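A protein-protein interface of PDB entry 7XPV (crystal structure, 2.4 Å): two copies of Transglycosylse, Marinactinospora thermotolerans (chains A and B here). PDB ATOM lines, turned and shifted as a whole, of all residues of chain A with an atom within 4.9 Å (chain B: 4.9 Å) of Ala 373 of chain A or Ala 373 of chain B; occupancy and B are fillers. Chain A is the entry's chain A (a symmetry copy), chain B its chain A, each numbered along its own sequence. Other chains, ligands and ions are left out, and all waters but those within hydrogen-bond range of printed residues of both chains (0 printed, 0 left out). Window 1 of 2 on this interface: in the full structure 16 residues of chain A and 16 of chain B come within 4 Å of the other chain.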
ATOM      1  N   GLN A 267     -17.027 -27.998  23.280  1.00  0.00           N
ATOM      2  CA  GLN A 267     -16.051 -27.009  23.714  1.00  0.00           C
ATOM      3  C   GLN A 267     -14.772 -27.154  22.909  1.00  0.00           C
ATOM      4  O   GLN A 267     -14.249 -28.271  22.784  1.00  0.00           O
ATOM      5  CB  GLN A 267     -15.747 -27.172  25.198  1.00  0.00           C
ATOM      6  CG  GLN A 267     -15.142 -25.942  25.837  1.00  0.00           C
ATOM      7  CD  GLN A 267     -16.051 -25.331  26.881  1.00  0.00           C
ATOM      8  OE1 GLN A 267     -17.274 -25.331  26.736  1.00  0.00           O
ATOM      9  NE2 GLN A 267     -15.457 -24.815  27.948  1.00  0.00           N
ATOM     10  N   PRO A 369      -5.132 -22.616  27.195  1.00  0.00           N
ATOM     11  CA  PRO A 369      -6.106 -21.912  28.052  1.00  0.00           C
ATOM     12  C   PRO A 369      -7.552 -22.338  27.840  1.00  0.00           C
ATOM     13  O   PRO A 369      -8.316 -22.394  28.810  1.00  0.00           O
ATOM     14  CB  PRO A 369      -5.886 -20.442  27.676  1.00  0.00           C
ATOM     15  CG  PRO A 369      -4.452 -20.381  27.307  1.00  0.00           C
ATOM     16  CD  PRO A 369      -4.157 -21.680  26.604  1.00  0.00           C
ATOM     17  N   ASP A 370      -7.951 -22.642  26.603  1.00  0.00           N
ATOM     18  CA  ASP A 370      -9.316 -23.103  26.373  1.00  0.00           C
ATOM     19  C   ASP A 370      -9.517 -24.542  26.832  1.00  0.00           C
ATOM     20  O   ASP A 370     -10.631 -24.912  27.216  1.00  0.00           O
ATOM     21  CB  ASP A 370      -9.691 -22.959  24.896  1.00  0.00           C
ATOM     22  CG  ASP A 370      -8.737 -23.691  23.971  1.00  0.00           C
ATOM     23  OD1 ASP A 370      -7.572 -23.904  24.363  1.00  0.00           O
ATOM     24  OD2 ASP A 370      -9.152 -24.044  22.847  1.00  0.00           O
ATOM     25  N   ALA A 371      -8.462 -25.359  26.808  1.00  0.00           N
ATOM     26  CA  ALA A 371      -8.585 -26.729  27.297  1.00  0.00           C
ATOM     27  C   ALA A 371      -8.777 -26.756  28.809  1.00  0.00           C
ATOM     28  O   ALA A 371      -9.569 -27.554  29.327  1.00  0.00           O
ATOM     29  CB  ALA A 371      -7.359 -27.547  26.893  1.00  0.00           C
ATOM     30  N   ARG A 372      -8.063 -25.889  29.533  1.00  0.00           N
ATOM     31  CA  ARG A 372      -8.276 -25.780  30.972  1.00  0.00           C
ATOM     32  C   ARG A 372      -9.654 -25.208  31.281  1.00  0.00           C
ATOM     33  O   ARG A 372     -10.312 -25.640  32.233  1.00  0.00           O
ATOM     34  CB  ARG A 372      -7.179 -24.920  31.598  1.00  0.00           C
ATOM     35  CG  ARG A 372      -5.768 -25.422  31.328  1.00  0.00           C
ATOM     36  CD  ARG A 372      -4.729 -24.485  31.919  1.00  0.00           C
ATOM     37  NE  ARG A 372      -3.369 -24.917  31.621  1.00  0.00           N
ATOM     38  CZ  ARG A 372      -2.636 -25.686  32.415  1.00  0.00           C
ATOM     39  NH1 ARG A 372      -3.105 -26.136  33.567  1.00  0.00           N
ATOM     40  NH2 ARG A 372      -1.399 -26.009  32.045  1.00  0.00           N
ATOM     41  N   ALA A 373     -10.110 -24.241  30.480  1.00  0.00           N
ATOM     42  CA  ALA A 373     -11.436 -23.666  30.675  1.00  0.00           C
ATOM     43  C   ALA A 373     -12.551 -24.679  30.453  1.00  0.00           C
ATOM     44  O   ALA A 373     -13.647 -24.496  30.994  1.00  0.00           O
ATOM     45  CB  ALA A 373     -11.633 -22.470  29.745  1.00  0.00           C
ATOM     46  N   PHE A 374     -12.301 -25.731  29.666  1.00  0.00           N
ATOM     47  CA  PHE A 374     -13.302 -26.779  29.485  1.00  0.00           C
ATOM     48  C   PHE A 374     -13.679 -27.420  30.816  1.00  0.00           C
ATOM     49  O   PHE A 374     -14.854 -27.715  31.060  1.00  0.00           O
ATOM     50  CB  PHE A 374     -12.789 -27.838  28.506  1.00  0.00           C
ATOM     51  CG  PHE A 374     -13.359 -29.214  28.740  1.00  0.00           C
ATOM     52  CD1 PHE A 374     -14.666 -29.510  28.386  1.00  0.00           C
ATOM     53  CD2 PHE A 374     -12.583 -30.212  29.311  1.00  0.00           C
ATOM     54  CE1 PHE A 374     -15.191 -30.774  28.603  1.00  0.00           C
ATOM     55  CE2 PHE A 374     -13.102 -31.479  29.529  1.00  0.00           C
ATOM     56  CZ  PHE A 374     -14.407 -31.759  29.174  1.00  0.00           C
ATOM     57  N   LEU A 375     -12.695 -27.643  31.691  1.00  0.00           N
ATOM     58  CA  LEU A 375     -12.992 -28.244  32.987  1.00  0.00           C
ATOM     59  C   LEU A 375     -13.730 -27.274  33.903  1.00  0.00           C
ATOM     60  O   LEU A 375     -14.557 -27.702  34.716  1.00  0.00           O
ATOM     61  CB  LEU A 375     -11.705 -28.729  33.654  1.00  0.00           C
ATOM     62  CG  LEU A 375     -10.980 -29.899  32.981  1.00  0.00           C
ATOM     63  CD1 LEU A 375      -9.687 -30.240  33.712  1.00  0.00           C
ATOM     64  CD2 LEU A 375     -11.887 -31.119  32.896  1.00  0.00           C
ATOM     65  N   HIS A 376     -13.452 -25.974  33.786  1.00  0.00           N
ATOM     66  CA  HIS A 376     -14.114 -25.004  34.654  1.00  0.00           C
ATOM     67  C   HIS A 376     -15.584 -24.843  34.286  1.00  0.00           C
ATOM     68  O   HIS A 376     -16.446 -24.778  35.171  1.00  0.00           O
ATOM     69  CB  HIS A 376     -13.392 -23.659  34.591  1.00  0.00           C
ATOM     70  CG  HIS A 376     -12.015 -23.684  35.180  1.00  0.00           C
ATOM     71  ND1 HIS A 376     -11.789 -23.735  36.538  1.00  0.00           N
ATOM     72  CD2 HIS A 376     -10.794 -23.664  34.595  1.00  0.00           C
ATOM     73  CE1 HIS A 376     -10.488 -23.748  36.766  1.00  0.00           C
ATOM     74  NE2 HIS A 376      -9.861 -23.704  35.604  1.00  0.00           N
ATOM     75  N   ARG A 377     -15.894 -24.778  32.990  1.00  0.00           N
ATOM     76  CA  ARG A 377     -17.290 -24.638  32.587  1.00  0.00           C
ATOM     77  C   ARG A 377     -18.065 -25.928  32.828  1.00  0.00           C
ATOM     78  O   ARG A 377     -19.234 -25.887  33.229  1.00  0.00           O
ATOM     79  CB  ARG A 377     -17.378 -24.216  31.120  1.00  0.00           C
ATOM     80  CG  ARG A 377     -18.800 -23.969  30.639  1.00  0.00           C
ATOM     81  CD  ARG A 377     -18.819 -23.140  29.365  1.00  0.00           C
ATOM     82  NE  ARG A 377     -20.180 -22.849  28.928  1.00  0.00           N
ATOM     83  CZ  ARG A 377     -20.811 -23.499  27.962  1.00  0.00           C
ATOM     84  NH1 ARG A 377     -20.226 -24.477  27.289  1.00  0.00           N
ATOM     85  NH2 ARG A 377     -22.060 -23.156  27.658  1.00  0.00           N
ATOM     86  N   SER A 378     -17.430 -27.081  32.599  1.00  0.00           N
ATOM     87  CA  SER A 378     -18.090 -28.354  32.880  1.00  0.00           C
ATOM     88  C   SER A 378     -18.425 -28.483  34.359  1.00  0.00           C
ATOM     89  O   SER A 378     -19.485 -29.006  34.720  1.00  0.00           O
ATOM     90  CB  SER A 378     -17.206 -29.521  32.436  1.00  0.00           C
ATOM     91  OG  SER A 378     -16.942 -29.474  31.046  1.00  0.00           O
ATOM     92  N   GLN B 267      -6.988 -15.924  26.942  1.00  0.00           N
ATOM     93  CA  GLN B 267      -8.015 -16.918  26.660  1.00  0.00           C
ATOM     94  C   GLN B 267      -8.576 -16.703  25.266  1.00  0.00           C
ATOM     95  O   GLN B 267      -8.946 -15.570  24.921  1.00  0.00           O
ATOM     96  CB  GLN B 267      -9.139 -16.835  27.686  1.00  0.00           C
ATOM     97  CG  GLN B 267      -9.981 -18.088  27.773  1.00  0.00           C
ATOM     98  CD  GLN B 267      -9.850 -18.775  29.114  1.00  0.00           C
ATOM     99  OE1 GLN B 267      -8.777 -18.789  29.719  1.00  0.00           O
ATOM    100  NE2 GLN B 267     -10.949 -19.340  29.594  1.00  0.00           N
ATOM    101  N   PRO B 369     -18.801 -21.298  22.774  1.00  0.00           N
ATOM    102  CA  PRO B 369     -18.507 -22.068  23.998  1.00  0.00           C
ATOM    103  C   PRO B 369     -17.223 -21.657  24.704  1.00  0.00           C
ATOM    104  O   PRO B 369     -17.178 -21.672  25.940  1.00  0.00           O
ATOM    105  CB  PRO B 369     -18.436 -23.510  23.481  1.00  0.00           C
ATOM    106  CG  PRO B 369     -19.376 -23.522  22.335  1.00  0.00           C
ATOM    107  CD  PRO B 369     -19.224 -22.179  21.670  1.00  0.00           C
ATOM    108  N   ASP B 370     -16.177 -21.291  23.961  1.00  0.00           N
ATOM    109  CA  ASP B 370     -14.948 -20.843  24.607  1.00  0.00           C
ATOM    110  C   ASP B 370     -15.083 -19.437  25.178  1.00  0.00           C
ATOM    111  O   ASP B 370     -14.417 -19.110  26.166  1.00  0.00           O
ATOM    112  CB  ASP B 370     -13.772 -20.909  23.629  1.00  0.00           C
ATOM    113  CG  ASP B 370     -14.011 -20.107  22.364  1.00  0.00           C
ATOM    114  OD1 ASP B 370     -15.186 -19.894  22.005  1.00  0.00           O
ATOM    115  OD2 ASP B 370     -13.020 -19.697  21.723  1.00  0.00           O
ATOM    116  N   ALA B 371     -15.936 -18.600  24.584  1.00  0.00           N
ATOM    117  CA  ALA B 371     -16.151 -17.263  25.129  1.00  0.00           C
ATOM    118  C   ALA B 371     -16.888 -17.327  26.462  1.00  0.00           C
ATOM    119  O   ALA B 371     -16.568 -16.575  27.392  1.00  0.00           O
ATOM    120  CB  ALA B 371     -16.918 -16.400  24.129  1.00  0.00           C
ATOM    121  N   ARG B 372     -17.873 -18.220  26.575  1.00  0.00           N
ATOM    122  CA  ARG B 372     -18.549 -18.416  27.853  1.00  0.00           C
ATOM    123  C   ARG B 372     -17.608 -19.031  28.882  1.00  0.00           C
ATOM    124  O   ARG B 372     -17.645 -18.667  30.062  1.00  0.00           O
ATOM    125  CB  ARG B 372     -19.788 -19.290  27.662  1.00  0.00           C
ATOM    126  CG  ARG B 372     -20.778 -18.747  26.641  1.00  0.00           C
ATOM    127  CD  ARG B 372     -21.947 -19.697  26.450  1.00  0.00           C
ATOM    128  NE  ARG B 372     -22.879 -19.223  25.434  1.00  0.00           N
ATOM    129  CZ  ARG B 372     -23.953 -18.487  25.686  1.00  0.00           C
ATOM    130  NH1 ARG B 372     -24.262 -18.113  26.916  1.00  0.00           N
ATOM    131  NH2 ARG B 372     -24.739 -18.120  24.677  1.00  0.00           N
ATOM    132  N   ALA B 373     -16.749 -19.958  28.449  1.00  0.00           N
ATOM    133  CA  ALA B 373     -15.782 -20.569  29.355  1.00  0.00           C
ATOM    134  C   ALA B 373     -14.770 -19.566  29.892  1.00  0.00           C
ATOM    135  O   ALA B 373     -14.200 -19.800  30.963  1.00  0.00           O
ATOM    136  CB  ALA B 373     -15.053 -21.713  28.652  1.00  0.00           C
ATOM    137  N   PHE B 374     -14.528 -18.465  29.171  1.00  0.00           N
ATOM    138  CA  PHE B 374     -13.633 -17.428  29.676  1.00  0.00           C
ATOM    139  C   PHE B 374     -14.125 -16.872  31.007  1.00  0.00           C
ATOM    140  O   PHE B 374     -13.325 -16.614  31.913  1.00  0.00           O
ATOM    141  CB  PHE B 374     -13.490 -16.305  28.646  1.00  0.00           C
ATOM    142  CG  PHE B 374     -13.193 -14.956  29.249  1.00  0.00           C
ATOM    143  CD1 PHE B 374     -11.935 -14.664  29.751  1.00  0.00           C
ATOM    144  CD2 PHE B 374     -14.175 -13.978  29.309  1.00  0.00           C
ATOM    145  CE1 PHE B 374     -11.662 -13.425  30.309  1.00  0.00           C
ATOM    146  CE2 PHE B 374     -13.908 -12.735  29.864  1.00  0.00           C
ATOM    147  CZ  PHE B 374     -12.650 -12.460  30.363  1.00  0.00           C
ATOM    148  N   LEU B 375     -15.439 -16.681  31.145  1.00  0.00           N
ATOM    149  CA  LEU B 375     -15.975 -16.162  32.399  1.00  0.00           C
ATOM    150  C   LEU B 375     -15.900 -17.197  33.516  1.00  0.00           C
ATOM    151  O   LEU B 375     -15.720 -16.832  34.683  1.00  0.00           O
ATOM    152  CB  LEU B 375     -17.417 -15.692  32.206  1.00  0.00           C
ATOM    153  CG  LEU B 375     -17.627 -14.471  31.303  1.00  0.00           C
ATOM    154  CD1 LEU B 375     -19.108 -14.149  31.150  1.00  0.00           C
ATOM    155  CD2 LEU B 375     -16.868 -13.266  31.840  1.00  0.00           C
ATOM    156  N   HIS B 376     -16.032 -18.482  33.183  1.00  0.00           N
ATOM    157  CA  HIS B 376     -15.990 -19.513  34.216  1.00  0.00           C
ATOM    158  C   HIS B 376     -14.584 -19.680  34.778  1.00  0.00           C
ATOM    159  O   HIS B 376     -14.408 -19.813  35.995  1.00  0.00           O
ATOM    160  CB  HIS B 376     -16.511 -20.839  33.663  1.00  0.00           C
ATOM    161  CG  HIS B 376     -17.970 -20.821  33.327  1.00  0.00           C
ATOM    162  ND1 HIS B 376     -18.955 -20.844  34.291  1.00  0.00           N
ATOM    163  CD2 HIS B 376     -18.611 -20.784  32.135  1.00  0.00           C
ATOM    164  CE1 HIS B 376     -20.140 -20.820  33.708  1.00  0.00           C
ATOM    165  NE2 HIS B 376     -19.960 -20.785  32.400  1.00  0.00           N
ATOM    166  N   ARG B 377     -13.568 -19.676  33.913  1.00  0.00           N
ATOM    167  CA  ARG B 377     -12.200 -19.819  34.402  1.00  0.00           C
ATOM    168  C   ARG B 377     -11.741 -18.560  35.128  1.00  0.00           C
ATOM    169  O   ARG B 377     -11.032 -18.646  36.137  1.00  0.00           O
ATOM    170  CB  ARG B 377     -11.257 -20.157  33.248  1.00  0.00           C
ATOM    171  CG  ARG B 377      -9.820 -20.402  33.684  1.00  0.00           C
ATOM    172  CD  ARG B 377      -9.038 -21.157  32.622  1.00  0.00           C
ATOM    173  NE  ARG B 377      -7.676 -21.448  33.055  1.00  0.00           N
ATOM    174  CZ  ARG B 377      -6.608 -20.755  32.686  1.00  0.00           C
ATOM    175  NH1 ARG B 377      -6.702 -19.729  31.855  1.00  0.00           N
ATOM    176  NH2 ARG B 377      -5.415 -21.104  33.158  1.00  0.00           N
ATOM    177  N   SER B 378     -12.139 -17.383  34.635  1.00  0.00           N
ATOM    178  CA  SER B 378     -11.798 -16.141  35.324  1.00  0.00           C
ATOM    179  C   SER B 378     -12.401 -16.104  36.721  1.00  0.00           C
ATOM    180  O   SER B 378     -11.767 -15.623  37.667  1.00  0.00           O
ATOM    181  CB  SER B 378     -12.271 -14.934  34.513  1.00  0.00           C
ATOM    182  OG  SER B 378     -11.664 -14.896  33.234  1.00  0.00           O
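Gln 267 of chain A touches Pro 369 of chain B, and with the chains exchanged Pro 369 of chain A touches Gln 267 of chain B. Gln 267 of chain A touches Ala 373 of chain B, and with the chains exchanged Ala 373 of chain A touches Gln 267 of chain B. Arg 372 of chain A touches Arg 377 of chain B, and with the chains exchanged Arg 377 of chain A touches Arg 372 of chain B. His 376 of chain A touches Arg 377 of chain B, and with the chains exchanged Arg 377 of chain A touches His 376 of chain B.
Printed residues of chain B within 4 Å of Ala 373 of chain A: Gln 267 (3.2 Å), Ala 373 (3.7 Å) and Arg 377 (3.9 Å). Of the printed residues of chain B, Arg 372 of chain A touches Arg 377 (3.7 Å). Of the printed residues of chain B, Pro 369 of chain A touches Gln 267. Printed residues of chain B within 4 Å of His 376 of chain A: Arg 377. Of the printed residues of chain A, Arg 372 of chain B touches Arg 377. Ala 371 of chain A touches none of the printed residues of chain B. The nearest printed residue of chain A that does not touch Ala 373 of chain B is Phe 374 of chain A (5.0 Å).
Of the 11 printed residues of chain A, 6 touch a printed residue of chain B. Of the 11 printed residues of chain B, 6 touch a printed residue of chain A. Printed residues of chain B that touch a printed residue of chain A: Gln 267, Pro 369, Arg 372, Ala 373, His 376 and Arg 377. Hydrophobic or aromatic side chains of chain B that line the printed part of chain A: Pro 369, Ala 373 and His 376. Among the printed residues, no Asp or Glu carboxylate lies within 4 Å of a Lys or Arg side-chain nitrogen of the other chain.
The guanidinium group (NH1) of Arg 377 of chain A sits at hydrogen-bond distance from the side-chain amide oxygen (OE1) of Gln 267 of chain A. The side-chain amide oxygen (OE1) of Gln 267 of chain B lies within hydrogen-bond range of the guanidinium group (NH1) of Arg 377 of chain B (3.1 Å).
Pro 369 of chain B touches Gln 267 of chain A. CB of Ala 373 of chain B touches NE2 of Gln 267 of chain A (3.2 Å). Pro 369 of chain A touches Gln 267 of chain B (O to OE1, 3.7 Å). Arg 372 of chain A touches Arg 377 of chain B (CD to NH2, 3.7 Å). NE2 of Gln 267 of chain B touches CB of Ala 373 of chain A (3.2 Å). Ala 373 of chain A touches Ala 373 of chain B (CB to CB, 3.7 Å). Arg 377 of chain B touches Ala 373 of chain A. CD2 of His 376 of chain A touches CG of Arg 377 of chain B, 3.5 Å away. Arg 377 of chain A touches Arg 372 of chain B (NH2 to CD, 3.7 Å). CD of Arg 377 of chain A touches N of Ala 373 of chain B, at 3.9 Å.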
